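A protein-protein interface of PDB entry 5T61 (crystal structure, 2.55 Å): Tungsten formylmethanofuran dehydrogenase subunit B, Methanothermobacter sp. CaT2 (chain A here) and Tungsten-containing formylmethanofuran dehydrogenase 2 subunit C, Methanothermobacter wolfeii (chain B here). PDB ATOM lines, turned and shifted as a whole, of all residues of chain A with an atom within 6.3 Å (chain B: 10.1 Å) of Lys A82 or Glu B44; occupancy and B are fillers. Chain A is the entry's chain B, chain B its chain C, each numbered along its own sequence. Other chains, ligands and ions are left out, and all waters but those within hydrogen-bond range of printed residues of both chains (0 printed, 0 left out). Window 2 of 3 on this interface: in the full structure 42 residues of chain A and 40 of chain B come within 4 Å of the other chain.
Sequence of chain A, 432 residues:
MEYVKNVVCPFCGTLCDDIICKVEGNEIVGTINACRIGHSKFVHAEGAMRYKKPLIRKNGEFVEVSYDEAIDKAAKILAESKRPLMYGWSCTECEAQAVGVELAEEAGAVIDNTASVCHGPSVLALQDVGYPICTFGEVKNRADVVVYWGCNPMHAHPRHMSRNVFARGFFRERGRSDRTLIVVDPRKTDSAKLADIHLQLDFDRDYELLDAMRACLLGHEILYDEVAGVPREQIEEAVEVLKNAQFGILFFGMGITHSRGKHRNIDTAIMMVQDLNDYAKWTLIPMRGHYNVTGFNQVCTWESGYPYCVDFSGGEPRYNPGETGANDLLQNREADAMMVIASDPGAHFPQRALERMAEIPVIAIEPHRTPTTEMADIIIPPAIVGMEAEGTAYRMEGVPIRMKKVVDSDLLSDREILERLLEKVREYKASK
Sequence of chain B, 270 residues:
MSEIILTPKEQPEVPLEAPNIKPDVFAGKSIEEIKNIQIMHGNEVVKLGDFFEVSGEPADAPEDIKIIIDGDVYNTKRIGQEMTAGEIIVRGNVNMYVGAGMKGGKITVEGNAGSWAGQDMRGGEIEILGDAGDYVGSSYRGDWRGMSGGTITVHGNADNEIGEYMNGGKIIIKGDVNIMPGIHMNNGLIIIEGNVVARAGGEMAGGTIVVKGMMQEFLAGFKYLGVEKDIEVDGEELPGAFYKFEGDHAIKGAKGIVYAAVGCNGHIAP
Of chain A, only Lys A82 (3.0 Å) comes within 4 Å of Glu B44.
Of chain B, only Asn B43 (3.1 Å) comes within 4 Å of Ser A81.
Of the printed residues of chain B, Arg A83 touches Val B14 (3.9 Å).
Printed residues of chain A within 4 Å of Val B14: Arg A83.
Glu A80 touches none of the printed residues of chain B.
The nearest residue of chain B that does not touch Lys A82 is Val B14 (4.5 Å).
O of Lys A82 sits at hydrogen-bond distance from N of Asn B43, 2.9 Å away.
The side-chain amide nitrogen (ND2) of Asn B43 sits at hydrogen-bond distance from the backbone carbonyl oxygen (O) of Ser A81, at 3.1 Å.
NZ of Lys A82 is in salt-bridge range of OE1 of Glu B44 (3.0 Å).
O of Ala A107 is in hydrogen-bond range of ND2 of Asn B43 (3.1 Å).
Among the printed residues, pairs that only touch across the chains: Lys A82 with His B41, Lys A82 with Gly B42, Arg A83 with Val B14, Gly A108 with Asn B43, Ser A313 with Gly B42 and Ser A313 with Asn B43.
N of Arg A83 is in hydrogen-bond range of OD1 of Asp A336.
O of Pro B15 sits at hydrogen-bond distance from N of Gly B42.
The side-chain carboxylate of Asp A336 lies within hydrogen-bond range of the backbone NH of Lys A82, 3.0 Å away.
O of Val B14 sits close to NE2 of His B41 (3.3 Å).
The backbone carbonyl oxygen (O) of Ile A77 lies within hydrogen-bond range of the side-chain hydroxyl (OG) of Ser A81 (2.5 Å).
Of the 12 printed residues of chain A, 6 touch a printed residue of chain B.
Among the printed residues, Asp or Glu carboxylates within 4 Å of a Lys or Arg side-chain nitrogen of the other chain: Lys A82 with Glu B44 (3.0 Å).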
ATOM      1  N   ILE A  77      19.797  44.404  -6.699  1.00  0.00           N
ATOM      2  CA  ILE A  77      18.882  43.889  -5.684  1.00  0.00           C
ATOM      3  C   ILE A  77      18.201  42.618  -6.179  1.00  0.00           C
ATOM      4  O   ILE A  77      18.127  41.613  -5.464  1.00  0.00           O
ATOM      5  CB  ILE A  77      17.857  44.970  -5.294  1.00  0.00           C
ATOM      6  CG1 ILE A  77      18.528  46.064  -4.460  1.00  0.00           C
ATOM      7  CG2 ILE A  77      16.702  44.358  -4.521  1.00  0.00           C
ATOM      8  CD1 ILE A  77      17.689  47.310  -4.297  1.00  0.00           C
ATOM      9  N   LEU A  78      17.697  42.641  -7.416  1.00  0.00           N
ATOM     10  CA  LEU A  78      16.980  41.478  -7.927  1.00  0.00           C
ATOM     11  C   LEU A  78      17.926  40.315  -8.198  1.00  0.00           C
ATOM     12  O   LEU A  78      17.560  39.152  -7.993  1.00  0.00           O
ATOM     13  CB  LEU A  78      16.218  41.831  -9.202  1.00  0.00           C
ATOM     14  CG  LEU A  78      15.273  43.030  -9.231  1.00  0.00           C
ATOM     15  CD1 LEU A  78      14.844  43.228 -10.659  1.00  0.00           C
ATOM     16  CD2 LEU A  78      14.070  42.857  -8.324  1.00  0.00           C
ATOM     17  N   ALA A  79      19.138  40.607  -8.679  1.00  0.00           N
ATOM     18  CA  ALA A  79      20.105  39.549  -8.949  1.00  0.00           C
ATOM     19  C   ALA A  79      20.497  38.826  -7.666  1.00  0.00           C
ATOM     20  O   ALA A  79      20.545  37.590  -7.622  1.00  0.00           O
ATOM     21  CB  ALA A  79      21.342  40.127  -9.640  1.00  0.00           C
ATOM     22  N   GLU A  80      20.785  39.590  -6.610  1.00  0.00           N
ATOM     23  CA  GLU A  80      21.172  39.029  -5.320  1.00  0.00           C
ATOM     24  C   GLU A  80      20.004  38.405  -4.568  1.00  0.00           C
ATOM     25  O   GLU A  80      20.233  37.650  -3.616  1.00  0.00           O
ATOM     26  CB  GLU A  80      21.799  40.120  -4.441  1.00  0.00           C
ATOM     27  CG  GLU A  80      20.768  40.865  -3.596  1.00  0.00           C
ATOM     28  CD  GLU A  80      21.390  41.803  -2.588  1.00  0.00           C
ATOM     29  OE1 GLU A  80      22.609  42.044  -2.666  1.00  0.00           O
ATOM     30  OE2 GLU A  80      20.660  42.300  -1.710  1.00  0.00           O
ATOM     31  N   SER A  81      18.772  38.704  -4.964  1.00  0.00           N
ATOM     32  CA  SER A  81      17.604  38.249  -4.226  1.00  0.00           C
ATOM     33  C   SER A  81      17.313  36.779  -4.500  1.00  0.00           C
ATOM     34  O   SER A  81      17.527  36.267  -5.602  1.00  0.00           O
ATOM     35  CB  SER A  81      16.390  39.105  -4.572  1.00  0.00           C
ATOM     36  OG  SER A  81      16.515  40.380  -3.970  1.00  0.00           O
ATOM     37  N   LYS A  82      16.821  36.101  -3.468  1.00  0.00           N
ATOM     38  CA  LYS A  82      16.523  34.677  -3.524  1.00  0.00           C
ATOM     39  C   LYS A  82      15.048  34.373  -3.689  1.00  0.00           C
ATOM     40  O   LYS A  82      14.689  33.232  -4.009  1.00  0.00           O
ATOM     41  CB  LYS A  82      16.979  34.029  -2.229  1.00  0.00           C
ATOM     42  CG  LYS A  82      17.768  32.788  -2.368  1.00  0.00           C
ATOM     43  CD  LYS A  82      18.338  32.551  -1.011  1.00  0.00           C
ATOM     44  CE  LYS A  82      19.175  31.331  -0.962  1.00  0.00           C
ATOM     45  NZ  LYS A  82      20.433  31.651  -0.235  1.00  0.00           N
ATOM     46  N   ARG A  83      14.209  35.362  -3.495  1.00  0.00           N
ATOM     47  CA  ARG A  83      12.781  35.196  -3.672  1.00  0.00           C
ATOM     48  C   ARG A  83      12.168  36.547  -4.011  1.00  0.00           C
ATOM     49  O   ARG A  83      11.346  37.067  -3.248  1.00  0.00           O
ATOM     50  CB  ARG A  83      12.168  34.646  -2.388  1.00  0.00           C
ATOM     51  CG  ARG A  83      10.750  34.146  -2.583  1.00  0.00           C
ATOM     52  CD  ARG A  83      10.687  32.705  -3.107  1.00  0.00           C
ATOM     53  NE  ARG A  83       9.400  32.158  -2.721  1.00  0.00           N
ATOM     54  CZ  ARG A  83       8.795  31.165  -3.350  1.00  0.00           C
ATOM     55  NH1 ARG A  83       9.343  30.535  -4.409  1.00  0.00           N
ATOM     56  NH2 ARG A  83       7.604  30.752  -2.929  1.00  0.00           N
ATOM     57  N   PRO A  84      12.550  37.160  -5.129  1.00  0.00           N
ATOM     58  CA  PRO A  84      12.032  38.494  -5.444  1.00  0.00           C
ATOM     59  C   PRO A  84      10.594  38.439  -5.934  1.00  0.00           C
ATOM     60  O   PRO A  84      10.184  37.507  -6.632  1.00  0.00           O
ATOM     61  CB  PRO A  84      12.985  38.993  -6.537  1.00  0.00           C
ATOM     62  CG  PRO A  84      13.486  37.760  -7.189  1.00  0.00           C
ATOM     63  CD  PRO A  84      13.506  36.682  -6.146  1.00  0.00           C
ATOM     64  N   ALA A 107      15.492  36.246 -13.217  1.00  0.00           N
ATOM     65  CA  ALA A 107      15.796  36.490 -11.814  1.00  0.00           C
ATOM     66  C   ALA A 107      15.314  35.381 -10.888  1.00  0.00           C
ATOM     67  O   ALA A 107      15.532  35.474  -9.677  1.00  0.00           O
ATOM     68  CB  ALA A 107      15.189  37.823 -11.368  1.00  0.00           C
ATOM     69  N   GLY A 108      14.682  34.339 -11.420  1.00  0.00           N
ATOM     70  CA  GLY A 108      14.087  33.324 -10.563  1.00  0.00           C
ATOM     71  C   GLY A 108      13.007  33.886  -9.665  1.00  0.00           C
ATOM     72  O   GLY A 108      12.861  33.448  -8.516  1.00  0.00           O
ATOM     73  N   SER A 313      11.200  30.305  -9.634  1.00  0.00           N
ATOM     74  CA  SER A 313      12.356  29.964  -8.807  1.00  0.00           C
ATOM     75  C   SER A 313      13.013  28.657  -9.240  1.00  0.00           C
ATOM     76  O   SER A 313      14.245  28.551  -9.265  1.00  0.00           O
ATOM     77  CB  SER A 313      11.943  29.892  -7.335  1.00  0.00           C
ATOM     78  OG  SER A 313      10.988  28.869  -7.121  1.00  0.00           O
ATOM     79  N   ASP A 336      11.937  38.498  -0.116  1.00  0.00           N
ATOM     80  CA  ASP A 336      13.066  39.252   0.414  1.00  0.00           C
ATOM     81  C   ASP A 336      13.399  40.494  -0.404  1.00  0.00           C
ATOM     82  O   ASP A 336      14.361  41.195  -0.076  1.00  0.00           O
ATOM     83  CB  ASP A 336      14.302  38.346   0.530  1.00  0.00           C
ATOM     84  CG  ASP A 336      14.742  37.767  -0.803  1.00  0.00           C
ATOM     85  OD1 ASP A 336      14.015  37.933  -1.805  1.00  0.00           O
ATOM     86  OD2 ASP A 336      15.817  37.133  -0.846  1.00  0.00           O
ATOM     87  N   PRO B  12      15.297  29.375   7.488  1.00  0.00           N
ATOM     88  CA  PRO B  12      15.440  30.659   6.807  1.00  0.00           C
ATOM     89  C   PRO B  12      14.096  31.334   6.587  1.00  0.00           C
ATOM     90  O   PRO B  12      13.040  30.702   6.559  1.00  0.00           O
ATOM     91  CB  PRO B  12      16.093  30.276   5.472  1.00  0.00           C
ATOM     92  CG  PRO B  12      15.618  28.858   5.231  1.00  0.00           C
ATOM     93  CD  PRO B  12      15.299  28.232   6.555  1.00  0.00           C
ATOM     94  N   GLU B  13      14.157  32.664   6.459  1.00  0.00           N
ATOM     95  CA  GLU B  13      12.957  33.436   6.160  1.00  0.00           C
ATOM     96  C   GLU B  13      12.408  33.068   4.788  1.00  0.00           C
ATOM     97  O   GLU B  13      11.189  32.969   4.605  1.00  0.00           O
ATOM     98  CB  GLU B  13      13.279  34.925   6.234  1.00  0.00           C
ATOM     99  CG  GLU B  13      13.256  35.503   7.635  1.00  0.00           C
ATOM    100  CD  GLU B  13      13.666  36.961   7.658  1.00  0.00           C
ATOM    101  OE1 GLU B  13      13.793  37.557   6.566  1.00  0.00           O
ATOM    102  OE2 GLU B  13      13.861  37.511   8.761  1.00  0.00           O
ATOM    103  N   VAL B  14      13.293  32.856   3.818  1.00  0.00           N
ATOM    104  CA  VAL B  14      12.914  32.325   2.513  1.00  0.00           C
ATOM    105  C   VAL B  14      12.783  30.814   2.662  1.00  0.00           C
ATOM    106  O   VAL B  14      13.758  30.142   3.023  1.00  0.00           O
ATOM    107  CB  VAL B  14      13.936  32.704   1.431  1.00  0.00           C
ATOM    108  CG1 VAL B  14      13.618  31.989   0.133  1.00  0.00           C
ATOM    109  CG2 VAL B  14      13.957  34.214   1.225  1.00  0.00           C
ATOM    110  N   PRO B  15      11.612  30.241   2.399  1.00  0.00           N
ATOM    111  CA  PRO B  15      11.366  28.849   2.784  1.00  0.00           C
ATOM    112  C   PRO B  15      12.178  27.853   1.973  1.00  0.00           C
ATOM    113  O   PRO B  15      12.746  28.155   0.921  1.00  0.00           O
ATOM    114  CB  PRO B  15       9.866  28.669   2.521  1.00  0.00           C
ATOM    115  CG  PRO B  15       9.317  30.055   2.537  1.00  0.00           C
ATOM    116  CD  PRO B  15      10.386  30.890   1.913  1.00  0.00           C
ATOM    117  N   LEU B  16      12.232  26.643   2.514  1.00  0.00           N
ATOM    118  CA  LEU B  16      12.801  25.486   1.848  1.00  0.00           C
ATOM    119  C   LEU B  16      11.685  24.685   1.192  1.00  0.00           C
ATOM    120  O   LEU B  16      10.568  24.609   1.709  1.00  0.00           O
ATOM    121  CB  LEU B  16      13.552  24.582   2.832  1.00  0.00           C
ATOM    122  CG  LEU B  16      14.797  25.022   3.602  1.00  0.00           C
ATOM    123  CD1 LEU B  16      15.105  24.007   4.701  1.00  0.00           C
ATOM    124  CD2 LEU B  16      15.969  25.116   2.632  1.00  0.00           C
ATOM    125  N   GLU B  17      11.995  24.100   0.039  1.00  0.00           N
ATOM    126  CA  GLU B  17      11.179  23.049  -0.549  1.00  0.00           C
ATOM    127  C   GLU B  17      12.022  21.783  -0.547  1.00  0.00           C
ATOM    128  O   GLU B  17      13.105  21.759  -1.142  1.00  0.00           O
ATOM    129  CB  GLU B  17      10.734  23.417  -1.965  1.00  0.00           C
ATOM    130  CG  GLU B  17      10.064  24.776  -2.053  1.00  0.00           C
ATOM    131  CD  GLU B  17       9.308  24.972  -3.347  1.00  0.00           C
ATOM    132  OE1 GLU B  17       9.212  26.119  -3.819  1.00  0.00           O
ATOM    133  OE2 GLU B  17       8.815  23.974  -3.904  1.00  0.00           O
ATOM    134  N   ALA B  18      11.529  20.727   0.092  1.00  0.00           N
ATOM    135  CA  ALA B  18      12.303  19.497   0.277  1.00  0.00           C
ATOM    136  C   ALA B  18      11.476  18.271  -0.096  1.00  0.00           C
ATOM    137  O   ALA B  18      11.228  17.397   0.741  1.00  0.00           O
ATOM    138  CB  ALA B  18      12.811  19.399   1.713  1.00  0.00           C
ATOM    139  N   ILE B  37      21.874  15.327  -0.576  1.00  0.00           N
ATOM    140  CA  ILE B  37      20.607  15.394  -1.297  1.00  0.00           C
ATOM    141  C   ILE B  37      20.248  16.844  -1.591  1.00  0.00           C
ATOM    142  O   ILE B  37      20.410  17.731  -0.742  1.00  0.00           O
ATOM    143  CB  ILE B  37      19.508  14.688  -0.483  1.00  0.00           C
ATOM    144  CG1 ILE B  37      19.693  13.169  -0.538  1.00  0.00           C
ATOM    145  CG2 ILE B  37      18.120  15.073  -0.977  1.00  0.00           C
ATOM    146  CD1 ILE B  37      18.882  12.418   0.497  1.00  0.00           C
ATOM    147  N   GLN B  38      19.743  17.091  -2.800  1.00  0.00           N
ATOM    148  CA  GLN B  38      19.369  18.439  -3.208  1.00  0.00           C
ATOM    149  C   GLN B  38      18.003  18.825  -2.664  1.00  0.00           C
ATOM    150  O   GLN B  38      17.049  18.044  -2.707  1.00  0.00           O
ATOM    151  CB  GLN B  38      19.372  18.570  -4.733  1.00  0.00           C
ATOM    152  CG  GLN B  38      20.742  18.508  -5.391  1.00  0.00           C
ATOM    153  CD  GLN B  38      20.700  18.997  -6.830  1.00  0.00           C
ATOM    154  OE1 GLN B  38      19.625  19.232  -7.383  1.00  0.00           O
ATOM    155  NE2 GLN B  38      21.871  19.234  -7.411  1.00  0.00           N
ATOM    156  N   ILE B  39      17.919  20.053  -2.155  1.00  0.00           N
ATOM    157  CA  ILE B  39      16.662  20.693  -1.791  1.00  0.00           C
ATOM    158  C   ILE B  39      16.698  22.117  -2.330  1.00  0.00           C
ATOM    159  O   ILE B  39      17.748  22.631  -2.718  1.00  0.00           O
ATOM    160  CB  ILE B  39      16.425  20.700  -0.264  1.00  0.00           C
ATOM    161  CG1 ILE B  39      17.492  21.541   0.440  1.00  0.00           C
ATOM    162  CG2 ILE B  39      16.419  19.287   0.290  1.00  0.00           C
ATOM    163  CD1 ILE B  39      17.212  21.776   1.899  1.00  0.00           C
ATOM    164  N   MET B  40      15.539  22.763  -2.331  1.00  0.00           N
ATOM    165  CA  MET B  40      15.433  24.134  -2.805  1.00  0.00           C
ATOM    166  C   MET B  40      15.328  25.094  -1.627  1.00  0.00           C
ATOM    167  O   MET B  40      14.767  24.765  -0.579  1.00  0.00           O
ATOM    168  CB  MET B  40      14.219  24.312  -3.715  1.00  0.00           C
ATOM    169  CG  MET B  40      14.304  23.580  -5.047  1.00  0.00           C
ATOM    170  SD  MET B  40      15.706  24.087  -6.066  1.00  0.00           S
ATOM    171  CE  MET B  40      15.247  25.761  -6.505  1.00  0.00           C
ATOM    172  N   HIS B  41      15.928  26.274  -1.791  1.00  0.00           N
ATOM    173  CA  HIS B  41      15.821  27.395  -0.854  1.00  0.00           C
ATOM    174  C   HIS B  41      15.640  28.661  -1.691  1.00  0.00           C
ATOM    175  O   HIS B  41      16.620  29.294  -2.089  1.00  0.00           O
ATOM    176  CB  HIS B  41      17.018  27.484   0.070  1.00  0.00           C
ATOM    177  CG  HIS B  41      17.076  28.797   0.848  1.00  0.00           C
ATOM    178  ND1 HIS B  41      18.247  29.276   1.410  1.00  0.00           N
ATOM    179  CD2 HIS B  41      16.117  29.720   1.105  1.00  0.00           C
ATOM    180  CE1 HIS B  41      18.000  30.419   1.993  1.00  0.00           C
ATOM    181  NE2 HIS B  41      16.722  30.707   1.814  1.00  0.00           N
ATOM    182  N   GLY B  42      14.390  29.021  -1.973  1.00  0.00           N
ATOM    183  CA  GLY B  42      14.138  30.113  -2.899  1.00  0.00           C
ATOM    184  C   GLY B  42      14.536  29.710  -4.303  1.00  0.00           C
ATOM    185  O   GLY B  42      14.199  28.614  -4.763  1.00  0.00           O
ATOM    186  N   ASN B  43      15.269  30.583  -5.000  1.00  0.00           N
ATOM    187  CA  ASN B  43      15.736  30.291  -6.350  1.00  0.00           C
ATOM    188  C   ASN B  43      17.135  29.671  -6.375  1.00  0.00           C
ATOM    189  O   ASN B  43      17.787  29.671  -7.425  1.00  0.00           O
ATOM    190  CB  ASN B  43      15.685  31.557  -7.210  1.00  0.00           C
ATOM    191  CG  ASN B  43      16.546  32.680  -6.664  1.00  0.00           C
ATOM    192  OD1 ASN B  43      17.389  32.471  -5.793  1.00  0.00           O
ATOM    193  ND2 ASN B  43      16.318  33.891  -7.163  1.00  0.00           N
ATOM    194  N   GLU B  44      17.599  29.146  -5.243  1.00  0.00           N
ATOM    195  CA  GLU B  44      18.896  28.500  -5.130  1.00  0.00           C
ATOM    196  C   GLU B  44      18.718  27.000  -4.947  1.00  0.00           C
ATOM    197  O   GLU B  44      17.849  26.557  -4.190  1.00  0.00           O
ATOM    198  CB  GLU B  44      19.687  29.051  -3.937  1.00  0.00           C
ATOM    199  CG  GLU B  44      20.541  30.275  -4.209  1.00  0.00           C
ATOM    200  CD  GLU B  44      21.466  30.572  -3.041  1.00  0.00           C
ATOM    201  OE1 GLU B  44      21.603  29.691  -2.164  1.00  0.00           O
ATOM    202  OE2 GLU B  44      22.032  31.684  -2.975  1.00  0.00           O
ATOM    203  N   VAL B  45      19.549  26.220  -5.625  1.00  0.00           N
ATOM    204  CA  VAL B  45      19.670  24.796  -5.339  1.00  0.00           C
ATOM    205  C   VAL B  45      20.742  24.632  -4.272  1.00  0.00           C
ATOM    206  O   VAL B  45      21.851  25.161  -4.412  1.00  0.00           O
ATOM    207  CB  VAL B  45      20.021  24.002  -6.608  1.00  0.00           C
ATOM    208  CG1 VAL B  45      20.050  22.506  -6.309  1.00  0.00           C
ATOM    209  CG2 VAL B  45      19.039  24.319  -7.725  1.00  0.00           C
ATOM    210  N   VAL B  46      20.419  23.910  -3.200  1.00  0.00           N
ATOM    211  CA  VAL B  46      21.333  23.724  -2.081  1.00  0.00           C
ATOM    212  C   VAL B  46      21.284  22.267  -1.632  1.00  0.00           C
ATOM    213  O   VAL B  46      20.584  21.433  -2.212  1.00  0.00           O
ATOM    214  CB  VAL B  46      21.006  24.657  -0.893  1.00  0.00           C
ATOM    215  CG1 VAL B  46      21.150  26.122  -1.290  1.00  0.00           C
ATOM    216  CG2 VAL B  46      19.616  24.371  -0.348  1.00  0.00           C
ATOM    217  N   LYS B  47      22.028  21.974  -0.570  1.00  0.00           N
ATOM    218  CA  LYS B  47      22.140  20.632  -0.021  1.00  0.00           C
ATOM    219  C   LYS B  47      21.399  20.550   1.305  1.00  0.00           C
ATOM    220  O   LYS B  47      21.350  21.522   2.065  1.00  0.00           O
ATOM    221  CB  LYS B  47      23.609  20.216   0.157  1.00  0.00           C
ATOM    222  CG  LYS B  47      24.249  19.728  -1.138  1.00  0.00           C
ATOM    223  CD  LYS B  47      25.735  19.404  -1.028  1.00  0.00           C
ATOM    224  CE  LYS B  47      26.604  20.613  -1.306  1.00  0.00           C
ATOM    225  NZ  LYS B  47      27.795  20.196  -2.098  1.00  0.00           N
ATOM    226  N   LEU B  48      20.793  19.385   1.553  1.00  0.00           N
ATOM    227  CA  LEU B  48      20.064  19.173   2.798  1.00  0.00           C
ATOM    228  C   LEU B  48      20.966  19.402   4.002  1.00  0.00           C
ATOM    229  O   LEU B  48      20.524  19.941   5.024  1.00  0.00           O
ATOM    230  CB  LEU B  48      19.472  17.761   2.819  1.00  0.00           C
ATOM    231  CG  LEU B  48      18.586  17.279   3.977  1.00  0.00           C
ATOM    232  CD1 LEU B  48      17.748  16.102   3.512  1.00  0.00           C
ATOM    233  CD2 LEU B  48      19.369  16.885   5.227  1.00  0.00           C
ATOM    234  N   ASP B  50      23.147  21.569   4.453  1.00  0.00           N
ATOM    235  CA  ASP B  50      23.301  22.990   4.740  1.00  0.00           C
ATOM    236  C   ASP B  50      22.264  23.498   5.733  1.00  0.00           C
ATOM    237  O   ASP B  50      22.457  24.567   6.324  1.00  0.00           O
ATOM    238  CB  ASP B  50      23.216  23.793   3.442  1.00  0.00           C
ATOM    239  CG  ASP B  50      24.354  23.482   2.492  1.00  0.00           C
ATOM    240  OD1 ASP B  50      25.459  23.151   2.972  1.00  0.00           O
ATOM    241  OD2 ASP B  50      24.137  23.552   1.264  1.00  0.00           O
ATOM    242  N   PHE B  51      21.165  22.771   5.920  1.00  0.00           N
ATOM    243  CA  PHE B  51      20.124  23.192   6.843  1.00  0.00           C
ATOM    244  C   PHE B  51      19.719  22.112   7.836  1.00  0.00           C
ATOM    245  O   PHE B  51      18.813  22.349   8.644  1.00  0.00           O
ATOM    246  CB  PHE B  51      18.890  23.672   6.063  1.00  0.00           C
ATOM    247  CG  PHE B  51      19.104  24.973   5.342  1.00  0.00           C
ATOM    248  CD1 PHE B  51      18.831  26.175   5.972  1.00  0.00           C
ATOM    249  CD2 PHE B  51      19.593  24.999   4.045  1.00  0.00           C
ATOM    250  CE1 PHE B  51      19.030  27.379   5.321  1.00  0.00           C
ATOM    251  CE2 PHE B  51      19.796  26.199   3.388  1.00  0.00           C
ATOM    252  CZ  PHE B  51      19.513  27.392   4.028  1.00  0.00           C
